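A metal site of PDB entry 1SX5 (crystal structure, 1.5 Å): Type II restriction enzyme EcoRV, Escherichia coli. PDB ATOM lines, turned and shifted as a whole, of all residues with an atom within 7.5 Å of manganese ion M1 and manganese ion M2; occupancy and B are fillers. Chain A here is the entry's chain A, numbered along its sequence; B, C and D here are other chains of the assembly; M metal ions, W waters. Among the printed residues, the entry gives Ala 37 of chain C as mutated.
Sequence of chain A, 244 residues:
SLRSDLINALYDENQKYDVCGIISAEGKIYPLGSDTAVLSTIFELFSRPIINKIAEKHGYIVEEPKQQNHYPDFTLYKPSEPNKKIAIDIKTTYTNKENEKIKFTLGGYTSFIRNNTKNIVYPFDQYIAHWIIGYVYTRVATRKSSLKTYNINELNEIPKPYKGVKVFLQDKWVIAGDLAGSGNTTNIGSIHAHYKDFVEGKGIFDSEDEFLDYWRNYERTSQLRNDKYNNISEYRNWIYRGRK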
ATOM      1  N   SER A  40       8.357   0.920   9.115  1.00  0.00           N
ATOM      2  CA  SER A  40       9.318   1.258   8.081  1.00  0.00           C
ATOM      3  C   SER A  40       9.183   0.287   6.904  1.00  0.00           C
ATOM      4  O   SER A  40       9.276   0.673   5.753  1.00  0.00           O
ATOM      5  CB  SER A  40      10.760   1.270   8.635  1.00  0.00           C
ATOM      6  OG  SER A  40      11.109  -0.004   9.096  1.00  0.00           O
ATOM      7  N   THR A  41       8.924  -0.973   7.179  1.00  0.00           N
ATOM      8  CA  THR A  41       8.770  -1.940   6.093  1.00  0.00           C
ATOM      9  C   THR A  41       7.494  -1.601   5.321  1.00  0.00           C
ATOM     10  O   THR A  41       7.523  -1.550   4.098  1.00  0.00           O
ATOM     11  CB  THR A  41       8.631  -3.313   6.700  1.00  0.00           C
ATOM     12  OG1 THR A  41       9.932  -3.664   7.191  1.00  0.00           O
ATOM     13  CG2 THR A  41       8.107  -4.328   5.670  1.00  0.00           C
ATOM     14  N   GLU A  44       7.692   1.561   3.121  1.00  0.00           N
ATOM     15  CA  GLU A  44       8.513   1.324   1.942  1.00  0.00           C
ATOM     16  C   GLU A  44       7.748   0.495   0.947  1.00  0.00           C
ATOM     17  O   GLU A  44       7.732   0.845  -0.243  1.00  0.00           O
ATOM     18  CB  GLU A  44       9.845   0.650   2.287  1.00  0.00           C
ATOM     19  CG  GLU A  44      10.723   1.590   3.022  1.00  0.00           C
ATOM     20  CD  GLU A  44      12.243   1.207   3.004  1.00  0.00           C
ATOM     21  OE1 GLU A  44      12.631   0.209   2.321  1.00  0.00           O
ATOM     22  OE2 GLU A  44      13.041   1.949   3.635  1.00  0.00           O
ATOM     23  N   GLU A  64      15.785  -1.790  -7.981  1.00  0.00           N
ATOM     24  CA  GLU A  64      15.941  -1.946  -6.550  1.00  0.00           C
ATOM     25  C   GLU A  64      17.218  -2.772  -6.415  1.00  0.00           C
ATOM     26  O   GLU A  64      17.643  -3.406  -7.383  1.00  0.00           O
ATOM     27  CB  GLU A  64      14.736  -2.686  -5.952  1.00  0.00           C
ATOM     28  CG  GLU A  64      13.450  -1.919  -6.048  1.00  0.00           C
ATOM     29  CD  GLU A  64      12.323  -2.681  -5.404  1.00  0.00           C
ATOM     30  OE1 GLU A  64      11.968  -2.387  -4.229  1.00  0.00           O
ATOM     31  OE2 GLU A  64      11.813  -3.583  -6.075  1.00  0.00           O
ATOM     32  N   PRO A  65      17.865  -2.732  -5.237  1.00  0.00           N
ATOM     33  CA  PRO A  65      19.099  -3.499  -4.988  1.00  0.00           C
ATOM     34  C   PRO A  65      18.888  -4.980  -5.256  1.00  0.00           C
ATOM     35  O   PRO A  65      17.930  -5.587  -4.771  1.00  0.00           O
ATOM     36  CB  PRO A  65      19.385  -3.252  -3.520  1.00  0.00           C
ATOM     37  CG  PRO A  65      18.793  -1.894  -3.238  1.00  0.00           C
ATOM     38  CD  PRO A  65      17.477  -1.959  -4.040  1.00  0.00           C
ATOM     39  N   HIS A  70      22.695  -2.886   0.241  1.00  0.00           N
ATOM     40  CA  HIS A  70      23.139  -1.890  -0.741  1.00  0.00           C
ATOM     41  C   HIS A  70      22.165  -0.777  -0.892  1.00  0.00           C
ATOM     42  O   HIS A  70      20.961  -0.986  -1.068  1.00  0.00           O
ATOM     43  CB  HIS A  70      23.392  -2.522  -2.119  1.00  0.00           C
ATOM     44  CG  HIS A  70      24.645  -3.326  -2.184  1.00  0.00           C
ATOM     45  ND1 HIS A  70      24.845  -4.451  -1.415  1.00  0.00           N
ATOM     46  CD2 HIS A  70      25.773  -3.168  -2.926  1.00  0.00           C
ATOM     47  CE1 HIS A  70      26.030  -4.959  -1.681  1.00  0.00           C
ATOM     48  NE2 HIS A  70      26.615  -4.199  -2.589  1.00  0.00           N
ATOM     49  N   PRO A  72      20.820   2.574  -3.060  1.00  0.00           N
ATOM     50  CA  PRO A  72      19.633   3.109  -2.397  1.00  0.00           C
ATOM     51  C   PRO A  72      18.433   2.184  -2.570  1.00  0.00           C
ATOM     52  O   PRO A  72      18.487   1.284  -3.390  1.00  0.00           O
ATOM     53  CB  PRO A  72      19.406   4.425  -3.111  1.00  0.00           C
ATOM     54  CG  PRO A  72      19.755   4.015  -4.621  1.00  0.00           C
ATOM     55  CD  PRO A  72      20.927   3.102  -4.458  1.00  0.00           C
ATOM     56  N   ASP A  73      17.343   2.465  -1.853  1.00  0.00           N
ATOM     57  CA  ASP A  73      16.095   1.673  -1.996  1.00  0.00           C
ATOM     58  C   ASP A  73      15.679   1.639  -3.468  1.00  0.00           C
ATOM     59  O   ASP A  73      15.222   0.606  -3.951  1.00  0.00           O
ATOM     60  CB  ASP A  73      14.966   2.284  -1.189  1.00  0.00           C
ATOM     61  CG  ASP A  73      15.087   2.002   0.278  1.00  0.00           C
ATOM     62  OD1 ASP A  73      15.533   0.891   0.614  1.00  0.00           O
ATOM     63  OD2 ASP A  73      14.686   2.861   1.094  1.00  0.00           O
ATOM     64  N   PHE A  74      15.819   2.765  -4.169  1.00  0.00           N
ATOM     65  CA  PHE A  74      15.452   2.808  -5.579  1.00  0.00           C
ATOM     66  C   PHE A  74      16.426   3.655  -6.361  1.00  0.00           C
ATOM     67  O   PHE A  74      16.818   4.721  -5.927  1.00  0.00           O
ATOM     68  CB  PHE A  74      14.048   3.408  -5.783  1.00  0.00           C
ATOM     69  CG  PHE A  74      12.967   2.744  -4.950  1.00  0.00           C
ATOM     70  CD1 PHE A  74      12.273   1.642  -5.418  1.00  0.00           C
ATOM     71  CD2 PHE A  74      12.673   3.247  -3.670  1.00  0.00           C
ATOM     72  CE1 PHE A  74      11.270   1.022  -4.635  1.00  0.00           C
ATOM     73  CE2 PHE A  74      11.673   2.638  -2.855  1.00  0.00           C
ATOM     74  CZ  PHE A  74      10.971   1.533  -3.344  1.00  0.00           C
ATOM     75  N   ILE A  88      16.879   7.162  -4.571  1.00  0.00           N
ATOM     76  CA  ILE A  88      15.777   7.497  -3.682  1.00  0.00           C
ATOM     77  C   ILE A  88      15.823   6.507  -2.523  1.00  0.00           C
ATOM     78  O   ILE A  88      15.792   5.314  -2.729  1.00  0.00           O
ATOM     79  CB  ILE A  88      14.412   7.359  -4.426  1.00  0.00           C
ATOM     80  CG1 ILE A  88      14.436   8.327  -5.620  1.00  0.00           C
ATOM     81  CG2 ILE A  88      13.244   7.771  -3.496  1.00  0.00           C
ATOM     82  CD1 ILE A  88      13.157   8.305  -6.434  1.00  0.00           C
ATOM     83  N   ASP A  89      15.901   7.021  -1.297  1.00  0.00           N
ATOM     84  CA  ASP A  89      15.971   6.123  -0.154  1.00  0.00           C
ATOM     85  C   ASP A  89      14.783   6.515   0.735  1.00  0.00           C
ATOM     86  O   ASP A  89      14.552   7.707   0.997  1.00  0.00           O
ATOM     87  CB  ASP A  89      17.321   6.393   0.534  1.00  0.00           C
ATOM     88  CG  ASP A  89      17.984   5.191   1.159  1.00  0.00           C
ATOM     89  OD1 ASP A  89      17.735   4.024   0.728  1.00  0.00           O
ATOM     90  OD2 ASP A  89      18.844   5.474   2.042  1.00  0.00           O
ATOM     91  N   ILE A  90      14.049   5.506   1.200  1.00  0.00           N
ATOM     92  CA  ILE A  90      12.910   5.749   2.071  1.00  0.00           C
ATOM     93  C   ILE A  90      13.331   5.644   3.543  1.00  0.00           C
ATOM     94  O   ILE A  90      14.021   4.697   3.921  1.00  0.00           O
ATOM     95  CB  ILE A  90      11.784   4.740   1.732  1.00  0.00           C
ATOM     96  CG1 ILE A  90      11.380   4.925   0.230  1.00  0.00           C
ATOM     97  CG2 ILE A  90      10.506   5.102   2.540  1.00  0.00           C
ATOM     98  CD1 ILE A  90      10.225   3.999  -0.147  1.00  0.00           C
ATOM     99  N   LYS A  91      12.982   6.613   4.381  1.00  0.00           N
ATOM    100  CA  LYS A  91      13.385   6.559   5.807  1.00  0.00           C
ATOM    101  C   LYS A  91      12.095   6.858   6.617  1.00  0.00           C
ATOM    102  O   LYS A  91      11.205   7.540   6.141  1.00  0.00           O
ATOM    103  CB  LYS A  91      14.460   7.595   6.137  1.00  0.00           C
ATOM    104  CG  LYS A  91      15.854   7.537   5.385  1.00  0.00           C
ATOM    105  CD  LYS A  91      16.527   6.203   5.638  1.00  0.00           C
ATOM    106  CE  LYS A  91      17.879   6.088   4.981  1.00  0.00           C
ATOM    107  NZ  LYS A  91      18.451   4.796   5.380  1.00  0.00           N
ATOM    108  N   THR A  92      11.998   6.300   7.825  1.00  0.00           N
ATOM    109  CA  THR A  92      10.805   6.467   8.619  1.00  0.00           C
ATOM    110  C   THR A  92      11.209   6.755  10.061  1.00  0.00           C
ATOM    111  O   THR A  92      12.265   6.273  10.552  1.00  0.00           O
ATOM    112  CB  THR A  92       9.992   5.130   8.612  1.00  0.00           C
ATOM    113  OG1 THR A  92       9.604   4.794   7.269  1.00  0.00           O
ATOM    114  CG2 THR A  92       8.808   5.171   9.503  1.00  0.00           C
ATOM    115  N   ILE A 133      12.686  10.041   0.828  1.00  0.00           N
ATOM    116  CA  ILE A 133      11.244  10.064   0.995  1.00  0.00           C
ATOM    117  C   ILE A 133      11.183   9.751   2.488  1.00  0.00           C
ATOM    118  O   ILE A 133      11.564   8.641   2.913  1.00  0.00           O
ATOM    119  CB  ILE A 133      10.552   8.957   0.240  1.00  0.00           C
ATOM    120  CG1 ILE A 133      10.532   9.371  -1.263  1.00  0.00           C
ATOM    121  CG2 ILE A 133       9.075   8.881   0.576  1.00  0.00           C
ATOM    122  CD1 ILE A 133       9.963   8.245  -2.236  1.00  0.00           C
ATOM    123  OP3  DA B   1      17.972   0.784   3.954  1.00  0.00           O
ATOM    124  P    DA B   1      16.763  -0.117   4.127  1.00  0.00           P
ATOM    125  OP1  DA B   1      16.918  -1.566   3.833  1.00  0.00           O
ATOM    126  OP2  DA B   1      15.502   0.445   3.447  1.00  0.00           O
ATOM    127  O5'  DA B   1      16.426   0.156   5.686  1.00  0.00           O
ATOM    128  C5'  DA B   1      17.038  -0.514   6.731  1.00  0.00           C
ATOM    129  C4'  DA B   1      16.383   0.022   7.956  1.00  0.00           C
ATOM    130  O4'  DA B   1      17.059  -0.516   9.069  1.00  0.00           O
ATOM    131  C3'  DA B   1      16.572   1.549   7.990  1.00  0.00           C
ATOM    132  O3'  DA B   1      15.374   2.250   8.261  1.00  0.00           O
ATOM    133  C2'  DA B   1      17.538   1.758   9.113  1.00  0.00           C
ATOM    134  C1'  DA B   1      17.351   0.517   9.931  1.00  0.00           C
ATOM    135  N9   DA B   1      18.600   0.138  10.472  1.00  0.00           N
ATOM    136  C8   DA B   1      19.868   0.370  10.012  1.00  0.00           C
ATOM    137  N7   DA B   1      20.767  -0.029  10.824  1.00  0.00           N
ATOM    138  C5   DA B   1      20.043  -0.571  11.882  1.00  0.00           C
ATOM    139  C6   DA B   1      20.409  -1.070  13.074  1.00  0.00           C
ATOM    140  N6   DA B   1      21.664  -1.042  13.521  1.00  0.00           N
ATOM    141  N1   DA B   1      19.441  -1.583  13.863  1.00  0.00           N
ATOM    142  C2   DA B   1      18.166  -1.487  13.467  1.00  0.00           C
ATOM    143  N3   DA B   1      17.689  -0.969  12.375  1.00  0.00           N
ATOM    144  C4   DA B   1      18.711  -0.524  11.624  1.00  0.00           C
ATOM    145  P    DT B   2      15.438   3.812   8.584  1.00  0.00           P
ATOM    146  OP1  DT B   2      14.239   4.328   7.921  1.00  0.00           O
ATOM    147  OP2  DT B   2      16.763   4.437   8.320  1.00  0.00           O
ATOM    148  O5'  DT B   2      15.179   3.853  10.162  1.00  0.00           O
ATOM    149  C5'  DT B   2      14.176   3.069  10.715  1.00  0.00           C
ATOM    150  C4'  DT B   2      14.285   3.130  12.220  1.00  0.00           C
ATOM    151  O4'  DT B   2      15.570   2.524  12.576  1.00  0.00           O
ATOM    152  C3'  DT B   2      14.307   4.541  12.811  1.00  0.00           C
ATOM    153  O3'  DT B   2      13.387   4.393  13.907  1.00  0.00           O
ATOM    154  C2'  DT B   2      15.764   4.719  13.252  1.00  0.00           C
ATOM    155  C1'  DT B   2      16.140   3.272  13.616  1.00  0.00           C
ATOM    156  N1   DT B   2      17.591   2.933  13.711  1.00  0.00           N
ATOM    157  C2   DT B   2      18.011   2.228  14.845  1.00  0.00           C
ATOM    158  O2   DT B   2      17.229   1.791  15.682  1.00  0.00           O
ATOM    159  N3   DT B   2      19.384   2.026  14.913  1.00  0.00           N
ATOM    160  C4   DT B   2      20.337   2.432  13.968  1.00  0.00           C
ATOM    161  O4   DT B   2      21.559   2.186  14.124  1.00  0.00           O
ATOM    162  C5   DT B   2      19.823   3.131  12.820  1.00  0.00           C
ATOM    163  C7   DT B   2      20.789   3.614  11.777  1.00  0.00           C
ATOM    164  C6   DT B   2      18.488   3.317  12.744  1.00  0.00           C
ATOM    165  N   ASP C  35      13.852  -6.897   0.332  1.00  0.00           N
ATOM    166  CA  ASP C  35      14.742  -6.536   1.429  1.00  0.00           C
ATOM    167  C   ASP C  35      14.596  -7.445   2.612  1.00  0.00           C
ATOM    168  O   ASP C  35      13.500  -7.832   2.952  1.00  0.00           O
ATOM    169  CB  ASP C  35      14.533  -5.127   1.923  1.00  0.00           C
ATOM    170  CG  ASP C  35      15.752  -4.643   2.606  1.00  0.00           C
ATOM    171  OD1 ASP C  35      15.854  -4.706   3.867  1.00  0.00           O
ATOM    172  OD2 ASP C  35      16.666  -4.236   1.848  1.00  0.00           O
ATOM    173  N   THR C  36      15.720  -7.759   3.250  1.00  0.00           N
ATOM    174  CA  THR C  36      15.765  -8.638   4.405  1.00  0.00           C
ATOM    175  C   THR C  36      14.786  -8.259   5.456  1.00  0.00           C
ATOM    176  O   THR C  36      14.108  -9.116   6.048  1.00  0.00           O
ATOM    177  CB  THR C  36      17.160  -8.612   5.000  1.00  0.00           C
ATOM    178  OG1 THR C  36      18.049  -9.098   4.000  1.00  0.00           O
ATOM    179  CG2 THR C  36      17.244  -9.503   6.268  1.00  0.00           C
ATOM    180  N   ALA C  37      14.685  -6.945   5.650  1.00  0.00           N
ATOM    181  CA  ALA C  37      13.775  -6.354   6.591  1.00  0.00           C
ATOM    182  C   ALA C  37      12.325  -6.811   6.329  1.00  0.00           C
ATOM    183  O   ALA C  37      11.564  -6.998   7.260  1.00  0.00           O
ATOM    184  CB  ALA C  37      13.885  -4.809   6.458  1.00  0.00           C
ATOM    185  N   VAL C  38      11.956  -6.975   5.060  1.00  0.00           N
ATOM    186  CA  VAL C  38      10.592  -7.312   4.698  1.00  0.00           C
ATOM    187  C   VAL C  38      10.147  -8.665   5.230  1.00  0.00           C
ATOM    188  O   VAL C  38       9.095  -8.785   5.832  1.00  0.00           O
ATOM    189  CB  VAL C  38      10.441  -7.338   3.146  1.00  0.00           C
ATOM    190  CG1 VAL C  38       9.001  -7.736   2.761  1.00  0.00           C
ATOM    191  CG2 VAL C  38      10.725  -5.945   2.598  1.00  0.00           C
ATOM    192  P    DT D   6      25.555   1.702   4.934  1.00  0.00           P
ATOM    193  OP1  DT D   6      25.570   2.660   3.810  1.00  0.00           O
ATOM    194  OP2  DT D   6      25.401   2.224   6.291  1.00  0.00           O
ATOM    195  O5'  DT D   6      24.242   0.781   4.777  1.00  0.00           O
ATOM    196  C5'  DT D   6      23.958   0.168   3.490  1.00  0.00           C
ATOM    197  C4'  DT D   6      22.626  -0.532   3.541  1.00  0.00           C
ATOM    198  O4'  DT D   6      22.748  -1.551   4.572  1.00  0.00           O
ATOM    199  C3'  DT D   6      21.452   0.368   3.972  1.00  0.00           C
ATOM    200  O3'  DT D   6      20.301   0.175   3.103  1.00  0.00           O
ATOM    201  C2'  DT D   6      21.132  -0.095   5.376  1.00  0.00           C
ATOM    202  C1'  DT D   6      21.638  -1.526   5.436  1.00  0.00           C
ATOM    203  N1   DT D   6      22.136  -1.830   6.789  1.00  0.00           N
ATOM    204  C2   DT D   6      21.530  -2.778   7.568  1.00  0.00           C
ATOM    205  O2   DT D   6      20.674  -3.531   7.143  1.00  0.00           O
ATOM    206  N3   DT D   6      22.004  -2.845   8.870  1.00  0.00           N
ATOM    207  C4   DT D   6      23.030  -2.079   9.429  1.00  0.00           C
ATOM    208  O4   DT D   6      23.294  -2.182  10.621  1.00  0.00           O
ATOM    209  C5   DT D   6      23.675  -1.178   8.486  1.00  0.00           C
ATOM    210  C7   DT D   6      24.838  -0.344   8.905  1.00  0.00           C
ATOM    211  C6   DT D   6      23.204  -1.101   7.245  1.00  0.00           C
HETATM  212 MN    MN M   1      14.804   2.583   3.408  1.00  0.00          MN
HETATM  213 MN    MN M   2      14.652  -0.662   1.816  1.00  0.00          MN
HETATM  214  O   HOH W   1      14.583  -1.619   0.010  1.00  0.00           O
HETATM  215  O   HOH W   2      15.286   2.458   5.474  1.00  0.00           O
HETATM  216  O   HOH W   3      16.591   3.134   3.234  1.00  0.00           O
HETATM  217  O   HOH W   4      17.366  -0.280   1.631  1.00  0.00           O
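O3' of DT 6 of chain D lies close to OP3 of DA 1 of chain B, 2.6 Å away. N of Asp 73 is in hydrogen-bond range of OD1 of Asp 89, at 3.0 Å. The backbone NH (N) of Asp 73 lies within hydrogen-bond range of the backbone carbonyl oxygen (O) of Ile 88 (3.4 Å).
Of the 22 residues printed, 4 come within 4 Å of manganese ion M1.
Of the 22 residues printed, 3 come within 4 Å of manganese ion M2. The nearest printed residue that does not touch manganese ion M2 is Asp 35 of chain C (4.1 Å).
Manganese ion M1 is bound by water W3 (1.9 Å), OE2 of Glu 44 (1.9 Å), water W2 (2.1 Å), OP2 of DA 1 of chain B (2.2 Å), O of Ile 90 (2.3 Å) and OD2 of Asp 73 (2.3 Å). Manganese ion M1 has six donor atoms within binding distance.
Manganese ion M2 is bound by water W1 (2.0 Å), OP2 of DA 1 of chain B (2.1 Å), the side-chain carboxylate (OD1) of Asp 73 (2.2 Å) and the side-chain carboxylate (OE1) of Glu 44 (2.3 Å). Manganese ion M2 has four donor atoms within binding distance. Slightly farther from manganese ion M2 lies water W4 (2.7 Å).
Water W3 lies within hydrogen-bond range of OP3 of DA 1 of chain B (2.8 Å), OD1 of Asp 89 (2.9 Å) and NZ of Lys 91 (3.3 Å). Water W4 bridges OP1 of DA 1 of chain B and O3' of DT 6 of chain D.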
